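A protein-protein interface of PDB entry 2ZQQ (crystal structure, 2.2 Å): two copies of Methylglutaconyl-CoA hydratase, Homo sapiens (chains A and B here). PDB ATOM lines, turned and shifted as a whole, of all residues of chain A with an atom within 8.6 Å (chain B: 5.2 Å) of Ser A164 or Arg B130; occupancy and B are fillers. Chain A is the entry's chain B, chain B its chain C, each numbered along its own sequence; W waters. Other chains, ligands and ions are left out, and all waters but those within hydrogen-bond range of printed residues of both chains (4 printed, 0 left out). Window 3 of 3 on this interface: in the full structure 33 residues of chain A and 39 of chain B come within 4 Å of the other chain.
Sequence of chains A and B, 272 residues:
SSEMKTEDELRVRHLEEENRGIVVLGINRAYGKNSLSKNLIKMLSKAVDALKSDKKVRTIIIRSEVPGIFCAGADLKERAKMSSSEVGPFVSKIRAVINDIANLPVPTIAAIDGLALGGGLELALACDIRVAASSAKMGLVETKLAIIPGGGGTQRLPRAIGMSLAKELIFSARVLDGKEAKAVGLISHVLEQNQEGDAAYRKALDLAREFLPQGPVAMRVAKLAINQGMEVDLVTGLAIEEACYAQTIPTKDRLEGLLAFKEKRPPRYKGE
Water W1 lies within hydrogen-bond range of the side-chain carboxylate (OE1) of Glu A168, the side-chain hydroxyl (OG) of Ser B188 and the backbone carbonyl oxygen (O) of Ser A164. Water W3 lies within hydrogen-bond range of the side-chain hydroxyl (OG) of Ser B188 (2.7 Å), the side-chain hydroxyl (OG) of Ser A164 (2.8 Å) and the backbone NH (N) of Arg B130 (3.0 Å). Water W2 lies within hydrogen-bond range of OD1 of Asp B128 (2.9 Å) and NZ of Lys A167 (3.0 Å). Water W4 bridges a ring nitrogen (NE2) of His B189 and the side-chain carboxylate (OE1) of Glu A168.
No position is printed for both chains.
Printed residues of chain A within 4 Å of Asp B128: Ser A164, Lys A167 and Phe A171. Of the printed residues of chain A, Arg B130 touches Ser A164 (3.9 Å). No residue of chain A comes within 4 Å of Val B131. Of the printed residues of chain A, Ser B188 touches Ser A164 and Glu A168. The nearest printed residue of chain B that does not touch Ser A164 is Cys B127 (5.6 Å).
OD1 of Asp B128 is in salt-bridge range of NZ of Lys A167, at 2.6 Å. The side-chain carboxylate (OE2) of Glu A168 lies within hydrogen-bond range of a ring nitrogen (NE2) of His B189 (2.8 Å). O of Asp B128 sits at hydrogen-bond distance from OG of Ser A164.
The guanidinium group of Arg B130 lies within hydrogen-bond range of the backbone carbonyl oxygen of Cys B127, at 2.9 Å. O of Leu B186 lies within hydrogen-bond range of NE of Arg B130. OE2 of Glu A168 lies within salt-bridge range of NH1 of Arg A174 (2.8 Å). O of His B189 is in hydrogen-bond range of N of Ala B132 (2.9 Å). The backbone NH (N) of Ser B188 sits at hydrogen-bond distance from the backbone carbonyl oxygen (O) of Arg B130 (2.9 Å). O of Ala B124 lies within hydrogen-bond range of NH1 of Arg B130 (3.0 Å).
Among the printed residues, pairs that only touch across the chains: Ser A164 with Ser B188 (3.5 Å), Glu A168 with Ile B129 (3.6 Å), Phe A171 with Asp B128 (3.6 Å), Ser A164 with Arg B130 (3.9 Å), Ser A164 with Ile B129 (3.9 Å) and Glu A168 with Ser B188 (3.99 Å).
Hydrophobic or aromatic side chains of chain A within 4 Å of the printed part of chain B: Phe A171. Along chain A the printed residues that touch a printed residue of chain B span positions 164 to 171. Printed residues of chain B that touch a printed residue of chain A: Asp B128, Ile B129, Arg B130, Ser B188 and His B189. Hydrophobic or aromatic side chains of chain B within 4 Å of the printed part of chain A: Ile B129 and His B189. Along chain B the printed residues that touch a printed residue of chain A span positions 128 to 189. Among the printed residues, 9 pairs touch across the chains. Among the printed residues, Asp or Glu carboxylates within 4 Å of a Lys or Arg side-chain nitrogen of the other chain: Lys A167 with Asp B128.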
ATOM      1  N   LEU A 157     -16.535  13.674  31.486  1.00  0.00           N
ATOM      2  CA  LEU A 157     -17.909  13.349  31.869  1.00  0.00           C
ATOM      3  C   LEU A 157     -18.564  12.496  30.778  1.00  0.00           C
ATOM      4  O   LEU A 157     -19.151  11.451  31.067  1.00  0.00           O
ATOM      5  CB  LEU A 157     -18.731  14.633  32.127  1.00  0.00           C
ATOM      6  CG  LEU A 157     -20.179  14.421  32.623  1.00  0.00           C
ATOM      7  CD1 LEU A 157     -20.128  13.786  34.020  1.00  0.00           C
ATOM      8  CD2 LEU A 157     -20.965  15.746  32.683  1.00  0.00           C
ATOM      9  N   PRO A 158     -18.456  12.918  29.505  1.00  0.00           N
ATOM     10  CA  PRO A 158     -19.037  12.188  28.369  1.00  0.00           C
ATOM     11  C   PRO A 158     -18.463  10.776  28.226  1.00  0.00           C
ATOM     12  O   PRO A 158     -19.175   9.830  27.878  1.00  0.00           O
ATOM     13  CB  PRO A 158     -18.658  13.060  27.173  1.00  0.00           C
ATOM     14  CG  PRO A 158     -18.520  14.410  27.768  1.00  0.00           C
ATOM     15  CD  PRO A 158     -17.806  14.153  29.040  1.00  0.00           C
ATOM     16  N   ARG A 159     -17.163  10.643  28.473  1.00  0.00           N
ATOM     17  CA  ARG A 159     -16.519   9.345  28.369  1.00  0.00           C
ATOM     18  C   ARG A 159     -16.920   8.449  29.538  1.00  0.00           C
ATOM     19  O   ARG A 159     -16.788   7.239  29.461  1.00  0.00           O
ATOM     20  CB  ARG A 159     -14.994   9.503  28.330  1.00  0.00           C
ATOM     21  CG  ARG A 159     -14.488  10.143  27.060  1.00  0.00           C
ATOM     22  CD  ARG A 159     -12.992  10.369  27.096  1.00  0.00           C
ATOM     23  NE  ARG A 159     -12.441  10.583  25.759  1.00  0.00           N
ATOM     24  CZ  ARG A 159     -12.600  11.685  25.031  1.00  0.00           C
ATOM     25  NH1 ARG A 159     -13.302  12.710  25.492  1.00  0.00           N
ATOM     26  NH2 ARG A 159     -12.042  11.766  23.839  1.00  0.00           N
ATOM     27  N   ILE A 161     -20.194   8.747  31.286  1.00  0.00           N
ATOM     28  CA  ILE A 161     -21.611   8.432  31.329  1.00  0.00           C
ATOM     29  C   ILE A 161     -22.353   8.547  30.001  1.00  0.00           C
ATOM     30  O   ILE A 161     -23.588   8.454  29.962  1.00  0.00           O
ATOM     31  CB  ILE A 161     -22.313   9.309  32.389  1.00  0.00           C
ATOM     32  CG1 ILE A 161     -22.179  10.795  32.031  1.00  0.00           C
ATOM     33  CG2 ILE A 161     -21.673   9.065  33.742  1.00  0.00           C
ATOM     34  CD1 ILE A 161     -22.978  11.719  32.936  1.00  0.00           C
ATOM     35  N   GLY A 162     -21.602   8.730  28.919  1.00  0.00           N
ATOM     36  CA  GLY A 162     -22.217   8.833  27.610  1.00  0.00           C
ATOM     37  C   GLY A 162     -22.490  10.271  27.238  1.00  0.00           C
ATOM     38  O   GLY A 162     -22.705  11.120  28.102  1.00  0.00           O
ATOM     39  N   MET A 163     -22.482  10.566  25.951  1.00  0.00           N
ATOM     40  CA  MET A 163     -22.736  11.932  25.542  1.00  0.00           C
ATOM     41  C   MET A 163     -24.110  12.468  25.938  1.00  0.00           C
ATOM     42  O   MET A 163     -24.228  13.590  26.427  1.00  0.00           O
ATOM     43  CB  MET A 163     -22.541  12.075  24.035  1.00  0.00           C
ATOM     44  CG  MET A 163     -21.091  12.279  23.635  1.00  0.00           C
ATOM     45  SD  MET A 163     -20.934  12.912  21.959  1.00  0.00           S
ATOM     46  CE  MET A 163     -20.900  11.374  21.017  1.00  0.00           C
ATOM     47  N   SER A 164     -25.149  11.663  25.750  1.00  0.00           N
ATOM     48  CA  SER A 164     -26.500  12.121  26.058  1.00  0.00           C
ATOM     49  C   SER A 164     -26.646  12.657  27.478  1.00  0.00           C
ATOM     50  O   SER A 164     -27.126  13.772  27.664  1.00  0.00           O
ATOM     51  CB  SER A 164     -27.512  11.002  25.815  1.00  0.00           C
ATOM     52  OG  SER A 164     -28.800  11.550  25.594  1.00  0.00           O
ATOM     53  N   LEU A 165     -26.238  11.870  28.473  1.00  0.00           N
ATOM     54  CA  LEU A 165     -26.330  12.294  29.867  1.00  0.00           C
ATOM     55  C   LEU A 165     -25.370  13.429  30.187  1.00  0.00           C
ATOM     56  O   LEU A 165     -25.717  14.359  30.921  1.00  0.00           O
ATOM     57  CB  LEU A 165     -26.055  11.116  30.812  1.00  0.00           C
ATOM     58  CG  LEU A 165     -27.137  10.037  30.854  1.00  0.00           C
ATOM     59  CD1 LEU A 165     -26.657   8.821  31.649  1.00  0.00           C
ATOM     60  CD2 LEU A 165     -28.408  10.632  31.449  1.00  0.00           C
ATOM     61  N   ALA A 166     -24.160  13.348  29.647  1.00  0.00           N
ATOM     62  CA  ALA A 166     -23.160  14.377  29.878  1.00  0.00           C
ATOM     63  C   ALA A 166     -23.656  15.717  29.348  1.00  0.00           C
ATOM     64  O   ALA A 166     -23.542  16.737  30.027  1.00  0.00           O
ATOM     65  CB  ALA A 166     -21.850  13.994  29.204  1.00  0.00           C
ATOM     66  N   LYS A 167     -24.197  15.720  28.131  1.00  0.00           N
ATOM     67  CA  LYS A 167     -24.712  16.961  27.563  1.00  0.00           C
ATOM     68  C   LYS A 167     -25.858  17.500  28.404  1.00  0.00           C
ATOM     69  O   LYS A 167     -25.925  18.701  28.659  1.00  0.00           O
ATOM     70  CB  LYS A 167     -25.210  16.758  26.128  1.00  0.00           C
ATOM     71  CG  LYS A 167     -24.121  16.630  25.084  1.00  0.00           C
ATOM     72  CD  LYS A 167     -24.732  16.281  23.723  1.00  0.00           C
ATOM     73  CE  LYS A 167     -23.659  15.996  22.701  1.00  0.00           C
ATOM     74  NZ  LYS A 167     -24.237  15.662  21.375  1.00  0.00           N
ATOM     75  N   GLU A 168     -26.762  16.627  28.844  1.00  0.00           N
ATOM     76  CA  GLU A 168     -27.879  17.118  29.640  1.00  0.00           C
ATOM     77  C   GLU A 168     -27.401  17.788  30.919  1.00  0.00           C
ATOM     78  O   GLU A 168     -27.906  18.843  31.280  1.00  0.00           O
ATOM     79  CB  GLU A 168     -28.870  16.008  29.997  1.00  0.00           C
ATOM     80  CG  GLU A 168     -30.096  16.556  30.732  1.00  0.00           C
ATOM     81  CD  GLU A 168     -31.176  15.512  30.950  1.00  0.00           C
ATOM     82  OE1 GLU A 168     -31.274  14.581  30.118  1.00  0.00           O
ATOM     83  OE2 GLU A 168     -31.934  15.636  31.944  1.00  0.00           O
ATOM     84  N   LEU A 169     -26.431  17.186  31.599  1.00  0.00           N
ATOM     85  CA  LEU A 169     -25.909  17.779  32.828  1.00  0.00           C
ATOM     86  C   LEU A 169     -25.146  19.089  32.569  1.00  0.00           C
ATOM     87  O   LEU A 169     -25.245  20.037  33.356  1.00  0.00           O
ATOM     88  CB  LEU A 169     -25.001  16.784  33.553  1.00  0.00           C
ATOM     89  CG  LEU A 169     -25.711  15.519  34.050  1.00  0.00           C
ATOM     90  CD1 LEU A 169     -24.754  14.656  34.881  1.00  0.00           C
ATOM     91  CD2 LEU A 169     -26.909  15.932  34.895  1.00  0.00           C
ATOM     92  N   ILE A 170     -24.388  19.153  31.477  1.00  0.00           N
ATOM     93  CA  ILE A 170     -23.642  20.375  31.176  1.00  0.00           C
ATOM     94  C   ILE A 170     -24.578  21.486  30.663  1.00  0.00           C
ATOM     95  O   ILE A 170     -24.443  22.644  31.059  1.00  0.00           O
ATOM     96  CB  ILE A 170     -22.493  20.094  30.150  1.00  0.00           C
ATOM     97  CG1 ILE A 170     -21.398  19.274  30.837  1.00  0.00           C
ATOM     98  CG2 ILE A 170     -21.910  21.403  29.601  1.00  0.00           C
ATOM     99  CD1 ILE A 170     -20.323  18.744  29.899  1.00  0.00           C
ATOM    100  N   PHE A 171     -25.531  21.121  29.808  1.00  0.00           N
ATOM    101  CA  PHE A 171     -26.498  22.077  29.249  1.00  0.00           C
ATOM    102  C   PHE A 171     -27.432  22.650  30.325  1.00  0.00           C
ATOM    103  O   PHE A 171     -27.806  23.819  30.271  1.00  0.00           O
ATOM    104  CB  PHE A 171     -27.358  21.402  28.165  1.00  0.00           C
ATOM    105  CG  PHE A 171     -26.626  21.109  26.878  1.00  0.00           C
ATOM    106  CD1 PHE A 171     -27.123  20.163  25.990  1.00  0.00           C
ATOM    107  CD2 PHE A 171     -25.450  21.782  26.546  1.00  0.00           C
ATOM    108  CE1 PHE A 171     -26.466  19.883  24.789  1.00  0.00           C
ATOM    109  CE2 PHE A 171     -24.784  21.512  25.349  1.00  0.00           C
ATOM    110  CZ  PHE A 171     -25.296  20.556  24.466  1.00  0.00           C
ATOM    111  N   ARG A 174     -27.109  21.237  35.962  1.00  0.00           N
ATOM    112  CA  ARG A 174     -27.793  20.578  37.073  1.00  0.00           C
ATOM    113  C   ARG A 174     -26.863  20.007  38.144  1.00  0.00           C
ATOM    114  O   ARG A 174     -25.799  19.482  37.841  1.00  0.00           O
ATOM    115  CB  ARG A 174     -28.674  19.451  36.516  1.00  0.00           C
ATOM    116  CG  ARG A 174     -29.619  18.805  37.514  1.00  0.00           C
ATOM    117  CD  ARG A 174     -30.416  17.711  36.820  1.00  0.00           C
ATOM    118  NE  ARG A 174     -31.084  18.216  35.619  1.00  0.00           N
ATOM    119  CZ  ARG A 174     -31.463  17.458  34.592  1.00  0.00           C
ATOM    120  NH1 ARG A 174     -31.243  16.150  34.606  1.00  0.00           N
ATOM    121  NH2 ARG A 174     -32.055  18.011  33.541  1.00  0.00           N
ATOM    122  N   ILE B 109     -33.440  18.260  21.155  1.00  0.00           N
ATOM    123  CA  ILE B 109     -34.191  17.265  21.915  1.00  0.00           C
ATOM    124  C   ILE B 109     -35.222  16.575  21.026  1.00  0.00           C
ATOM    125  O   ILE B 109     -35.953  17.232  20.280  1.00  0.00           O
ATOM    126  CB  ILE B 109     -34.930  17.920  23.095  1.00  0.00           C
ATOM    127  CG1 ILE B 109     -33.944  18.726  23.945  1.00  0.00           C
ATOM    128  CG2 ILE B 109     -35.611  16.854  23.934  1.00  0.00           C
ATOM    129  CD1 ILE B 109     -34.606  19.561  25.049  1.00  0.00           C
ATOM    130  N   ALA B 110     -35.271  15.249  21.103  1.00  0.00           N
ATOM    131  CA  ALA B 110     -36.218  14.475  20.312  1.00  0.00           C
ATOM    132  C   ALA B 110     -37.395  14.070  21.192  1.00  0.00           C
ATOM    133  O   ALA B 110     -37.238  13.267  22.109  1.00  0.00           O
ATOM    134  CB  ALA B 110     -35.541  13.230  19.751  1.00  0.00           C
ATOM    135  N   ILE B 112     -40.478  12.000  21.450  1.00  0.00           N
ATOM    136  CA  ILE B 112     -41.124  10.868  20.795  1.00  0.00           C
ATOM    137  C   ILE B 112     -42.454  10.439  21.430  1.00  0.00           C
ATOM    138  O   ILE B 112     -42.473   9.700  22.418  1.00  0.00           O
ATOM    139  CB  ILE B 112     -40.158   9.658  20.763  1.00  0.00           C
ATOM    140  CG1 ILE B 112     -38.791  10.102  20.235  1.00  0.00           C
ATOM    141  CG2 ILE B 112     -40.711   8.572  19.857  1.00  0.00           C
ATOM    142  CD1 ILE B 112     -37.716   9.038  20.357  1.00  0.00           C
ATOM    143  N   ALA B 124     -33.831  10.605  15.623  1.00  0.00           N
ATOM    144  CA  ALA B 124     -33.832  10.899  17.049  1.00  0.00           C
ATOM    145  C   ALA B 124     -32.458  10.634  17.666  1.00  0.00           C
ATOM    146  O   ALA B 124     -32.072  11.282  18.642  1.00  0.00           O
ATOM    147  CB  ALA B 124     -34.902  10.062  17.759  1.00  0.00           C
ATOM    148  N   LEU B 125     -31.729   9.679  17.102  1.00  0.00           N
ATOM    149  CA  LEU B 125     -30.396   9.356  17.609  1.00  0.00           C
ATOM    150  C   LEU B 125     -29.446  10.506  17.321  1.00  0.00           C
ATOM    151  O   LEU B 125     -28.424  10.655  17.988  1.00  0.00           O
ATOM    152  CB  LEU B 125     -29.859   8.085  16.956  1.00  0.00           C
ATOM    153  CG  LEU B 125     -30.413   6.773  17.498  1.00  0.00           C
ATOM    154  CD1 LEU B 125     -30.001   5.636  16.575  1.00  0.00           C
ATOM    155  CD2 LEU B 125     -29.887   6.553  18.916  1.00  0.00           C
ATOM    156  N   ALA B 126     -29.806  11.313  16.324  1.00  0.00           N
ATOM    157  CA  ALA B 126     -29.015  12.459  15.916  1.00  0.00           C
ATOM    158  C   ALA B 126     -29.205  13.645  16.864  1.00  0.00           C
ATOM    159  O   ALA B 126     -28.458  14.619  16.794  1.00  0.00           O
ATOM    160  CB  ALA B 126     -29.378  12.858  14.479  1.00  0.00           C
ATOM    161  N   CYS B 127     -30.202  13.567  17.744  1.00  0.00           N
ATOM    162  CA  CYS B 127     -30.444  14.639  18.707  1.00  0.00           C
ATOM    163  C   CYS B 127     -29.642  14.381  19.978  1.00  0.00           C
ATOM    164  O   CYS B 127     -29.352  13.236  20.317  1.00  0.00           O
ATOM    165  CB  CYS B 127     -31.928  14.727  19.051  1.00  0.00           C
ATOM    166  SG  CYS B 127     -32.971  15.174  17.644  1.00  0.00           S
ATOM    167  N   ASP B 128     -29.288  15.442  20.691  1.00  0.00           N
ATOM    168  CA  ASP B 128     -28.512  15.281  21.910  1.00  0.00           C
ATOM    169  C   ASP B 128     -29.253  14.470  22.956  1.00  0.00           C
ATOM    170  O   ASP B 128     -28.681  13.581  23.575  1.00  0.00           O
ATOM    171  CB  ASP B 128     -28.146  16.642  22.510  1.00  0.00           C
ATOM    172  CG  ASP B 128     -27.340  17.496  21.566  1.00  0.00           C
ATOM    173  OD1 ASP B 128     -26.460  16.943  20.866  1.00  0.00           O
ATOM    174  OD2 ASP B 128     -27.578  18.727  21.527  1.00  0.00           O
ATOM    175  N   ILE B 129     -30.530  14.787  23.148  1.00  0.00           N
ATOM    176  CA  ILE B 129     -31.358  14.121  24.150  1.00  0.00           C
ATOM    177  C   ILE B 129     -32.686  13.593  23.595  1.00  0.00           C
ATOM    178  O   ILE B 129     -33.342  14.250  22.783  1.00  0.00           O
ATOM    179  CB  ILE B 129     -31.675  15.094  25.301  1.00  0.00           C
ATOM    180  CG1 ILE B 129     -30.370  15.601  25.913  1.00  0.00           C
ATOM    181  CG2 ILE B 129     -32.566  14.414  26.346  1.00  0.00           C
ATOM    182  CD1 ILE B 129     -30.549  16.754  26.870  1.00  0.00           C
ATOM    183  N   ARG B 130     -33.078  12.409  24.052  1.00  0.00           N
ATOM    184  CA  ARG B 130     -34.324  11.785  23.622  1.00  0.00           C
ATOM    185  C   ARG B 130     -35.272  11.538  24.793  1.00  0.00           C
ATOM    186  O   ARG B 130     -34.868  11.001  25.829  1.00  0.00           O
ATOM    187  CB  ARG B 130     -34.041  10.451  22.931  1.00  0.00           C
ATOM    188  CG  ARG B 130     -33.456  10.566  21.543  1.00  0.00           C
ATOM    189  CD  ARG B 130     -32.869   9.230  21.107  1.00  0.00           C
ATOM    190  NE  ARG B 130     -31.685   8.885  21.890  1.00  0.00           N
ATOM    191  CZ  ARG B 130     -30.541   9.570  21.859  1.00  0.00           C
ATOM    192  NH1 ARG B 130     -30.423  10.637  21.079  1.00  0.00           N
ATOM    193  NH2 ARG B 130     -29.514   9.191  22.608  1.00  0.00           N
ATOM    194  N   VAL B 131     -36.528  11.942  24.631  1.00  0.00           N
ATOM    195  CA  VAL B 131     -37.547  11.725  25.655  1.00  0.00           C
ATOM    196  C   VAL B 131     -38.739  11.043  24.978  1.00  0.00           C
ATOM    197  O   VAL B 131     -39.078  11.364  23.835  1.00  0.00           O
ATOM    198  CB  VAL B 131     -38.004  13.054  26.293  1.00  0.00           C
ATOM    199  CG1 VAL B 131     -36.819  13.748  26.932  1.00  0.00           C
ATOM    200  CG2 VAL B 131     -38.635  13.942  25.251  1.00  0.00           C
ATOM    201  N   ALA B 132     -39.374  10.103  25.671  1.00  0.00           N
ATOM    202  CA  ALA B 132     -40.504   9.397  25.076  1.00  0.00           C
ATOM    203  C   ALA B 132     -41.571   8.944  26.061  1.00  0.00           C
ATOM    204  O   ALA B 132     -41.314   8.804  27.258  1.00  0.00           O
ATOM    205  CB  ALA B 132     -40.000   8.190  24.291  1.00  0.00           C
ATOM    206  N   ALA B 160     -24.629   4.987  21.579  1.00  0.00           N
ATOM    207  CA  ALA B 160     -25.557   5.426  22.612  1.00  0.00           C
ATOM    208  C   ALA B 160     -25.841   4.360  23.664  1.00  0.00           C
ATOM    209  O   ALA B 160     -25.839   4.647  24.859  1.00  0.00           O
ATOM    210  CB  ALA B 160     -26.860   5.874  21.977  1.00  0.00           C
ATOM    211  N   LEU B 186     -31.670   4.026  25.789  1.00  0.00           N
ATOM    212  CA  LEU B 186     -31.908   4.547  24.443  1.00  0.00           C
ATOM    213  C   LEU B 186     -32.492   5.951  24.539  1.00  0.00           C
ATOM    214  O   LEU B 186     -32.321   6.774  23.637  1.00  0.00           O
ATOM    215  CB  LEU B 186     -32.862   3.627  23.669  1.00  0.00           C
ATOM    216  CG  LEU B 186     -33.301   4.073  22.264  1.00  0.00           C
ATOM    217  CD1 LEU B 186     -32.094   4.541  21.459  1.00  0.00           C
ATOM    218  CD2 LEU B 186     -34.012   2.912  21.555  1.00  0.00           C
ATOM    219  N   ILE B 187     -33.191   6.211  25.637  1.00  0.00           N
ATOM    220  CA  ILE B 187     -33.784   7.517  25.883  1.00  0.00           C
ATOM    221  C   ILE B 187     -33.413   7.899  27.307  1.00  0.00           C
ATOM    222  O   ILE B 187     -33.105   7.030  28.120  1.00  0.00           O
ATOM    223  CB  ILE B 187     -35.321   7.486  25.744  1.00  0.00           C
ATOM    224  CG1 ILE B 187     -35.918   6.527  26.777  1.00  0.00           C
ATOM    225  CG2 ILE B 187     -35.703   7.086  24.325  1.00  0.00           C
ATOM    226  CD1 ILE B 187     -37.418   6.433  26.716  1.00  0.00           C
ATOM    227  N   SER B 188     -33.447   9.192  27.610  1.00  0.00           N
ATOM    228  CA  SER B 188     -33.085   9.656  28.945  1.00  0.00           C
ATOM    229  C   SER B 188     -34.284   9.920  29.836  1.00  0.00           C
ATOM    230  O   SER B 188     -34.178   9.860  31.060  1.00  0.00           O
ATOM    231  CB  SER B 188     -32.241  10.923  28.845  1.00  0.00           C
ATOM    232  OG  SER B 188     -31.029  10.656  28.163  1.00  0.00           O
ATOM    233  N   HIS B 189     -35.424  10.216  29.226  1.00  0.00           N
ATOM    234  CA  HIS B 189     -36.634  10.491  29.992  1.00  0.00           C
ATOM    235  C   HIS B 189     -37.858   9.763  29.438  1.00  0.00           C
ATOM    236  O   HIS B 189     -38.122   9.771  28.232  1.00  0.00           O
ATOM    237  CB  HIS B 189     -36.909  12.001  30.021  1.00  0.00           C
ATOM    238  CG  HIS B 189     -35.841  12.799  30.707  1.00  0.00           C
ATOM    239  ND1 HIS B 189     -35.593  12.704  32.060  1.00  0.00           N
ATOM    240  CD2 HIS B 189     -34.953  13.704  30.224  1.00  0.00           C
ATOM    241  CE1 HIS B 189     -34.602  13.518  32.382  1.00  0.00           C
ATOM    242  NE2 HIS B 189     -34.195  14.135  31.286  1.00  0.00           N
HETATM  243  O   HOH W   1     -29.752  12.980  28.869  1.00  0.00           O
HETATM  244  O   HOH W   2     -25.166  15.964  18.494  1.00  0.00           O
HETATM  245  O   HOH W   3     -31.337  10.384  25.464  1.00  0.00           O
HETATM  246  O   HOH W   4     -31.770  12.287  32.457  1.00  0.00           O
